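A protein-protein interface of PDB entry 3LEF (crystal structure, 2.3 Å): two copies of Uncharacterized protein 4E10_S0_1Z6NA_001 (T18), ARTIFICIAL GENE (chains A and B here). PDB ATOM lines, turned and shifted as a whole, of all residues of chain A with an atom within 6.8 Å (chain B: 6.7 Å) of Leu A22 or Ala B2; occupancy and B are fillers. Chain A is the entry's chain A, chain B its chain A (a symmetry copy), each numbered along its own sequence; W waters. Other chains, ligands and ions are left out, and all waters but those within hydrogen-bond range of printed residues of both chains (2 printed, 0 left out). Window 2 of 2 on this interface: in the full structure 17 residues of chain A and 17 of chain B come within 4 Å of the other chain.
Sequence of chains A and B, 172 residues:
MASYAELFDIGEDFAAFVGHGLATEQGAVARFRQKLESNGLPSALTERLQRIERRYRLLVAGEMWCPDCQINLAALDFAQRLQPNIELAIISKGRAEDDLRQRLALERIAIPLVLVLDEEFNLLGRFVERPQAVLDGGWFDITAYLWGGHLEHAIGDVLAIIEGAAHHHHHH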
ATOM      1  N   VAL A  18     -18.275  -9.266 -21.943  1.00  0.00           N
ATOM      2  CA  VAL A  18     -17.171  -9.405 -20.986  1.00  0.00           C
ATOM      3  C   VAL A  18     -17.620  -9.854 -19.588  1.00  0.00           C
ATOM      4  O   VAL A  18     -16.960 -10.694 -18.951  1.00  0.00           O
ATOM      5  CB  VAL A  18     -16.331  -8.102 -20.916  1.00  0.00           C
ATOM      6  CG1 VAL A  18     -15.242  -8.215 -19.866  1.00  0.00           C
ATOM      7  CG2 VAL A  18     -15.712  -7.826 -22.290  1.00  0.00           C
ATOM      8  N   GLY A  19     -18.752  -9.325 -19.128  1.00  0.00           N
ATOM      9  CA  GLY A  19     -19.325  -9.702 -17.834  1.00  0.00           C
ATOM     10  C   GLY A  19     -19.753 -11.161 -17.676  1.00  0.00           C
ATOM     11  O   GLY A  19     -19.932 -11.637 -16.556  1.00  0.00           O
ATOM     12  N   HIS A  20     -19.917 -11.883 -18.780  1.00  0.00           N
ATOM     13  CA  HIS A  20     -20.245 -13.308 -18.730  1.00  0.00           C
ATOM     14  C   HIS A  20     -19.022 -14.197 -18.749  1.00  0.00           C
ATOM     15  O   HIS A  20     -19.147 -15.422 -18.692  1.00  0.00           O
ATOM     16  CB  HIS A  20     -21.114 -13.699 -19.928  1.00  0.00           C
ATOM     17  CG  HIS A  20     -22.494 -13.124 -19.891  1.00  0.00           C
ATOM     18  ND1 HIS A  20     -23.319 -13.246 -18.796  1.00  0.00           N
ATOM     19  CD2 HIS A  20     -23.204 -12.460 -20.830  1.00  0.00           C
ATOM     20  CE1 HIS A  20     -24.465 -12.641 -19.047  1.00  0.00           C
ATOM     21  NE2 HIS A  20     -24.421 -12.154 -20.276  1.00  0.00           N
ATOM     22  N   GLY A  21     -17.839 -13.603 -18.855  1.00  0.00           N
ATOM     23  CA  GLY A  21     -16.602 -14.376 -18.969  1.00  0.00           C
ATOM     24  C   GLY A  21     -16.038 -14.799 -17.631  1.00  0.00           C
ATOM     25  O   GLY A  21     -16.404 -14.259 -16.592  1.00  0.00           O
ATOM     26  N   LEU A  22     -15.148 -15.783 -17.655  1.00  0.00           N
ATOM     27  CA  LEU A  22     -14.482 -16.227 -16.441  1.00  0.00           C
ATOM     28  C   LEU A  22     -13.640 -15.076 -15.918  1.00  0.00           C
ATOM     29  O   LEU A  22     -13.282 -14.194 -16.678  1.00  0.00           O
ATOM     30  CB  LEU A  22     -13.593 -17.437 -16.732  1.00  0.00           C
ATOM     31  CG  LEU A  22     -14.296 -18.744 -17.062  1.00  0.00           C
ATOM     32  CD1 LEU A  22     -13.328 -19.748 -17.680  1.00  0.00           C
ATOM     33  CD2 LEU A  22     -14.917 -19.289 -15.803  1.00  0.00           C
ATOM     34  N   ALA A  23     -13.335 -15.076 -14.625  1.00  0.00           N
ATOM     35  CA  ALA A  23     -12.479 -14.058 -14.050  1.00  0.00           C
ATOM     36  C   ALA A  23     -11.151 -13.951 -14.809  1.00  0.00           C
ATOM     37  O   ALA A  23     -10.649 -12.849 -15.014  1.00  0.00           O
ATOM     38  CB  ALA A  23     -12.224 -14.352 -12.574  1.00  0.00           C
ATOM     39  N   THR A  24     -10.589 -15.093 -15.222  1.00  0.00           N
ATOM     40  CA  THR A  24      -9.314 -15.131 -15.965  1.00  0.00           C
ATOM     41  C   THR A  24      -9.410 -14.429 -17.330  1.00  0.00           C
ATOM     42  O   THR A  24      -8.492 -13.708 -17.744  1.00  0.00           O
ATOM     43  CB  THR A  24      -8.834 -16.580 -16.188  1.00  0.00           C
ATOM     44  OG1 THR A  24      -9.851 -17.339 -16.866  1.00  0.00           O
ATOM     45  CG2 THR A  24      -8.502 -17.251 -14.855  1.00  0.00           C
ATOM     46  N   GLU A  25     -10.531 -14.636 -18.012  1.00  0.00           N
ATOM     47  CA  GLU A  25     -10.749 -14.084 -19.344  1.00  0.00           C
ATOM     48  C   GLU A  25     -11.051 -12.586 -19.316  1.00  0.00           C
ATOM     49  O   GLU A  25     -10.697 -11.856 -20.251  1.00  0.00           O
ATOM     50  CB  GLU A  25     -11.917 -14.801 -19.993  1.00  0.00           C
ATOM     51  CG  GLU A  25     -11.776 -16.307 -20.020  1.00  0.00           C
ATOM     52  CD  GLU A  25     -13.053 -16.996 -20.435  1.00  0.00           C
ATOM     53  OE1 GLU A  25     -14.144 -16.377 -20.360  1.00  0.00           O
ATOM     54  OE2 GLU A  25     -12.969 -18.167 -20.845  1.00  0.00           O
ATOM     55  N   GLN A  26     -11.734 -12.139 -18.262  1.00  0.00           N
ATOM     56  CA  GLN A  26     -11.987 -10.724 -18.042  1.00  0.00           C
ATOM     57  C   GLN A  26     -10.677  -9.994 -17.731  1.00  0.00           C
ATOM     58  O   GLN A  26     -10.529  -8.812 -18.033  1.00  0.00           O
ATOM     59  CB  GLN A  26     -12.954 -10.542 -16.876  1.00  0.00           C
ATOM     60  CG  GLN A  26     -14.358 -11.011 -17.168  1.00  0.00           C
ATOM     61  CD  GLN A  26     -15.359 -10.499 -16.171  1.00  0.00           C
ATOM     62  OE1 GLN A  26     -15.299  -9.347 -15.760  1.00  0.00           O
ATOM     63  NE2 GLN A  26     -16.299 -11.339 -15.790  1.00  0.00           N
ATOM     64  N   GLY A  27      -9.734 -10.708 -17.125  1.00  0.00           N
ATOM     65  CA  GLY A  27      -8.412 -10.174 -16.860  1.00  0.00           C
ATOM     66  C   GLY A  27      -7.565 -10.064 -18.112  1.00  0.00           C
ATOM     67  O   GLY A  27      -6.772  -9.150 -18.229  1.00  0.00           O
ATOM     68  N   MET A  64     -15.825 -15.431 -25.097  1.00  0.00           N
ATOM     69  CA  MET A  64     -14.856 -14.828 -24.188  1.00  0.00           C
ATOM     70  C   MET A  64     -13.646 -15.703 -23.877  1.00  0.00           C
ATOM     71  O   MET A  64     -12.670 -15.230 -23.294  1.00  0.00           O
ATOM     72  CB  MET A  64     -15.536 -14.440 -22.880  1.00  0.00           C
ATOM     73  CG  MET A  64     -16.090 -13.032 -22.869  1.00  0.00           C
ATOM     74  SD  MET A  64     -14.763 -11.824 -22.864  1.00  0.00           S
ATOM     75  CE  MET A  64     -14.159 -11.961 -21.182  1.00  0.00           C
ATOM     76  N   TRP A  65     -13.687 -16.967 -24.264  1.00  0.00           N
ATOM     77  CA  TRP A  65     -12.589 -17.891 -23.962  1.00  0.00           C
ATOM     78  C   TRP A  65     -11.548 -17.908 -25.065  1.00  0.00           C
ATOM     79  O   TRP A  65     -10.443 -18.438 -24.890  1.00  0.00           O
ATOM     80  CB  TRP A  65     -13.136 -19.299 -23.743  1.00  0.00           C
ATOM     81  CG  TRP A  65     -14.075 -19.761 -24.836  1.00  0.00           C
ATOM     82  CD1 TRP A  65     -15.425 -19.851 -24.759  1.00  0.00           C
ATOM     83  CD2 TRP A  65     -13.716 -20.201 -26.159  1.00  0.00           C
ATOM     84  NE1 TRP A  65     -15.933 -20.322 -25.940  1.00  0.00           N
ATOM     85  CE2 TRP A  65     -14.903 -20.542 -26.817  1.00  0.00           C
ATOM     86  CE3 TRP A  65     -12.504 -20.338 -26.843  1.00  0.00           C
ATOM     87  CZ2 TRP A  65     -14.920 -21.028 -28.126  1.00  0.00           C
ATOM     88  CZ3 TRP A  65     -12.522 -20.805 -28.145  1.00  0.00           C
ATOM     89  CH2 TRP A  65     -13.730 -21.131 -28.775  1.00  0.00           C
ATOM     90  N   ALA B   2     -11.771 -24.435 -16.683  1.00  0.00           N
ATOM     91  CA  ALA B   2     -12.513 -23.958 -15.479  1.00  0.00           C
ATOM     92  C   ALA B   2     -13.193 -25.124 -14.759  1.00  0.00           C
ATOM     93  O   ALA B   2     -13.637 -26.054 -15.395  1.00  0.00           O
ATOM     94  CB  ALA B   2     -13.538 -22.923 -15.880  1.00  0.00           C
ATOM     95  N   SER B   3     -13.253 -25.066 -13.429  1.00  0.00           N
ATOM     96  CA  SER B   3     -13.983 -26.049 -12.626  1.00  0.00           C
ATOM     97  C   SER B   3     -15.480 -26.025 -12.937  1.00  0.00           C
ATOM     98  O   SER B   3     -15.980 -25.070 -13.507  1.00  0.00           O
ATOM     99  CB  SER B   3     -13.779 -25.764 -11.139  1.00  0.00           C
ATOM    100  OG  SER B   3     -14.513 -24.618 -10.716  1.00  0.00           O
ATOM    101  N   TYR B   4     -16.203 -27.070 -12.554  1.00  0.00           N
ATOM    102  CA  TYR B   4     -17.646 -27.097 -12.798  1.00  0.00           C
ATOM    103  C   TYR B   4     -18.357 -25.960 -12.063  1.00  0.00           C
ATOM    104  O   TYR B   4     -19.389 -25.482 -12.522  1.00  0.00           O
ATOM    105  CB  TYR B   4     -18.248 -28.442 -12.387  1.00  0.00           C
ATOM    106  CG  TYR B   4     -17.923 -29.592 -13.319  1.00  0.00           C
ATOM    107  CD1 TYR B   4     -17.538 -30.826 -12.823  1.00  0.00           C
ATOM    108  CD2 TYR B   4     -17.995 -29.439 -14.695  1.00  0.00           C
ATOM    109  CE1 TYR B   4     -17.246 -31.873 -13.671  1.00  0.00           C
ATOM    110  CE2 TYR B   4     -17.714 -30.482 -15.547  1.00  0.00           C
ATOM    111  CZ  TYR B   4     -17.334 -31.695 -15.035  1.00  0.00           C
ATOM    112  OH  TYR B   4     -17.043 -32.730 -15.903  1.00  0.00           O
ATOM    113  N   ALA B   5     -17.809 -25.544 -10.919  1.00  0.00           N
ATOM    114  CA  ALA B   5     -18.340 -24.409 -10.137  1.00  0.00           C
ATOM    115  C   ALA B   5     -18.145 -23.081 -10.858  1.00  0.00           C
ATOM    116  O   ALA B   5     -18.981 -22.178 -10.772  1.00  0.00           O
ATOM    117  CB  ALA B   5     -17.652 -24.336  -8.765  1.00  0.00           C
ATOM    118  N   GLU B   6     -17.017 -22.952 -11.538  1.00  0.00           N
ATOM    119  CA  GLU B   6     -16.699 -21.721 -12.228  1.00  0.00           C
ATOM    120  C   GLU B   6     -17.563 -21.613 -13.470  1.00  0.00           C
ATOM    121  O   GLU B   6     -18.052 -20.523 -13.796  1.00  0.00           O
ATOM    122  CB  GLU B   6     -15.204 -21.655 -12.566  1.00  0.00           C
ATOM    123  CG  GLU B   6     -14.328 -21.426 -11.338  1.00  0.00           C
ATOM    124  CD  GLU B   6     -12.857 -21.641 -11.608  1.00  0.00           C
ATOM    125  OE1 GLU B   6     -12.543 -22.312 -12.608  1.00  0.00           O
ATOM    126  OE2 GLU B   6     -12.020 -21.145 -10.814  1.00  0.00           O
ATOM    127  N   LEU B   7     -17.766 -22.746 -14.139  1.00  0.00           N
ATOM    128  CA  LEU B   7     -18.592 -22.794 -15.345  1.00  0.00           C
ATOM    129  C   LEU B   7     -20.069 -22.549 -15.046  1.00  0.00           C
ATOM    130  O   LEU B   7     -20.757 -21.852 -15.787  1.00  0.00           O
ATOM    131  CB  LEU B   7     -18.417 -24.137 -16.068  1.00  0.00           C
ATOM    132  CG  LEU B   7     -17.123 -24.294 -16.882  1.00  0.00           C
ATOM    133  CD1 LEU B   7     -17.102 -25.616 -17.628  1.00  0.00           C
ATOM    134  CD2 LEU B   7     -16.936 -23.142 -17.870  1.00  0.00           C
ATOM    135  N   ILE B  10     -20.769 -18.677 -14.429  1.00  0.00           N
ATOM    136  CA  ILE B  10     -20.907 -17.835 -15.619  1.00  0.00           C
ATOM    137  C   ILE B  10     -22.030 -18.312 -16.543  1.00  0.00           C
ATOM    138  O   ILE B  10     -22.370 -17.636 -17.519  1.00  0.00           O
ATOM    139  CB  ILE B  10     -19.569 -17.703 -16.444  1.00  0.00           C
ATOM    140  CG1 ILE B  10     -19.029 -19.061 -16.885  1.00  0.00           C
ATOM    141  CG2 ILE B  10     -18.517 -16.947 -15.659  1.00  0.00           C
ATOM    142  CD1 ILE B  10     -18.059 -18.969 -18.046  1.00  0.00           C
ATOM    143  N   ARG B  95     -18.090 -22.806 -25.773  1.00  0.00           N
ATOM    144  CA  ARG B  95     -17.347 -22.972 -24.511  1.00  0.00           C
ATOM    145  C   ARG B  95     -17.256 -24.426 -24.063  1.00  0.00           C
ATOM    146  O   ARG B  95     -16.303 -24.813 -23.395  1.00  0.00           O
ATOM    147  CB  ARG B  95     -17.988 -22.173 -23.388  1.00  0.00           C
ATOM    148  CG  ARG B  95     -17.238 -22.319 -22.085  1.00  0.00           C
ATOM    149  CD  ARG B  95     -17.751 -21.373 -21.027  1.00  0.00           C
ATOM    150  NE  ARG B  95     -17.562 -19.964 -21.349  1.00  0.00           N
ATOM    151  CZ  ARG B  95     -16.459 -19.265 -21.090  1.00  0.00           C
ATOM    152  NH1 ARG B  95     -15.407 -19.848 -20.540  1.00  0.00           N
ATOM    153  NH2 ARG B  95     -16.409 -17.979 -21.395  1.00  0.00           N
ATOM    154  N   ASP B  99     -13.707 -26.371 -23.430  1.00  0.00           N
ATOM    155  CA  ASP B  99     -13.303 -26.668 -22.049  1.00  0.00           C
ATOM    156  C   ASP B  99     -13.868 -27.961 -21.454  1.00  0.00           C
ATOM    157  O   ASP B  99     -13.330 -28.461 -20.463  1.00  0.00           O
ATOM    158  CB  ASP B  99     -13.640 -25.482 -21.130  1.00  0.00           C
ATOM    159  CG  ASP B  99     -12.768 -25.432 -19.877  1.00  0.00           C
ATOM    160  OD1 ASP B  99     -11.539 -25.650 -19.973  1.00  0.00           O
ATOM    161  OD2 ASP B  99     -13.311 -25.154 -18.788  1.00  0.00           O
ATOM    162  N   LEU B 100     -14.916 -28.523 -22.046  1.00  0.00           N
ATOM    163  CA  LEU B 100     -15.532 -29.722 -21.486  1.00  0.00           C
ATOM    164  C   LEU B 100     -15.256 -31.019 -22.278  1.00  0.00           C
ATOM    165  O   LEU B 100     -15.573 -32.127 -21.805  1.00  0.00           O
ATOM    166  CB  LEU B 100     -17.041 -29.506 -21.350  1.00  0.00           C
ATOM    167  CG  LEU B 100     -17.550 -28.556 -20.264  1.00  0.00           C
ATOM    168  CD1 LEU B 100     -19.068 -28.476 -20.337  1.00  0.00           C
ATOM    169  CD2 LEU B 100     -17.142 -29.055 -18.914  1.00  0.00           C
ATOM    170  N   ARG B 103     -12.278 -33.581 -20.451  1.00  0.00           N
ATOM    171  CA  ARG B 103     -12.691 -34.220 -19.206  1.00  0.00           C
ATOM    172  C   ARG B 103     -13.874 -35.186 -19.390  1.00  0.00           C
ATOM    173  O   ARG B 103     -13.970 -36.209 -18.688  1.00  0.00           O
ATOM    174  CB  ARG B 103     -13.008 -33.174 -18.132  1.00  0.00           C
ATOM    175  CG  ARG B 103     -14.301 -32.408 -18.328  1.00  0.00           C
ATOM    176  CD  ARG B 103     -14.456 -31.337 -17.260  1.00  0.00           C
ATOM    177  NE  ARG B 103     -13.813 -30.088 -17.648  1.00  0.00           N
ATOM    178  CZ  ARG B 103     -13.844 -28.967 -16.936  1.00  0.00           C
ATOM    179  NH1 ARG B 103     -14.482 -28.916 -15.777  1.00  0.00           N
ATOM    180  NH2 ARG B 103     -13.227 -27.892 -17.390  1.00  0.00           N
HETATM  181  O   HOH W   1     -19.029 -16.304 -21.051  1.00  0.00           O
HETATM  182  O   HOH W   2     -23.177 -15.135 -16.733  1.00  0.00           O
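NE1 of Trp A65 lies close to N of Arg B95, at 3.3 Å. The side-chain carboxylate of Glu A25 is in salt-bridge range of the guanidinium group of Arg B95 (3.0 Å).
The backbone NH (N) of Ser B3 sits at hydrogen-bond distance from the side-chain carboxylate (OE1) of Glu B6, at 3.0 Å. The side-chain carboxylate (OE1) of Glu A25 lies within hydrogen-bond range of the backbone NH (N) of Leu A22 (2.9 Å). The backbone carbonyl oxygen of Gly A21 lies within hydrogen-bond range of the side-chain amide nitrogen of Gln A26, at 3.0 Å. The backbone NH (N) of Ala B2 lies within hydrogen-bond range of the side-chain carboxylate (OD2) of Asp B99 (2.7 Å). The backbone carbonyl oxygen (O) of Ala B2 is in hydrogen-bond range of the guanidinium group (NH2) of Arg B103.
O of His A20 touches CB of Ile B10, 3.2 Å away. O of Gly A21 touches CG2 of Ile B10, 3.5 Å away. CB of Ala B2 touches CD1 of Leu A22 (3.7 Å). Leu A22 touches Glu B6. Ile B10 touches Leu A22. Leu A22 touches Arg B95. Arg B95 touches Met A64.
Leu A22 touches just these residues of chain B: Ala B2, Glu B6, Ile B10 and Arg B95. Of the printed residues of chain B, Met A64 touches Arg B95. Printed residues of chain B within 4 Å of Trp A65: Arg B95. Ala B2 touches just one residue of chain A: Leu A22 (3.7 Å). Printed residues of chain A within 4 Å of Ile B10: His A20 (3.2 Å), Gly A21 (3.5 Å) and Leu A22 (3.9 Å).
Printed residues of chain B that touch a printed residue of chain A: Ala B2, Glu B6, Ile B10 and Arg B95. Hydrophobic or aromatic side chains of chain B within 4 Å of the printed part of chain A: Ala B2 and Ile B10. Printed residues of chain A that touch a printed residue of chain B: His A20, Gly A21, Leu A22, Glu A25, Met A64 and Trp A65. Hydrophobic or aromatic side chains of chain A that line the printed part of chain B: Leu A22, Met A64 and Trp A65. Among the printed residues, 9 pairs touch across the chains.
No position is printed for both chains.
Water W1 lies within hydrogen-bond range of O of His A20 (2.5 Å) and NH2 of Arg B95 (3.1 Å). Water W2 bridges O of Ile B10 (2.7 Å) and ND1 of His A20 (2.8 Å).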
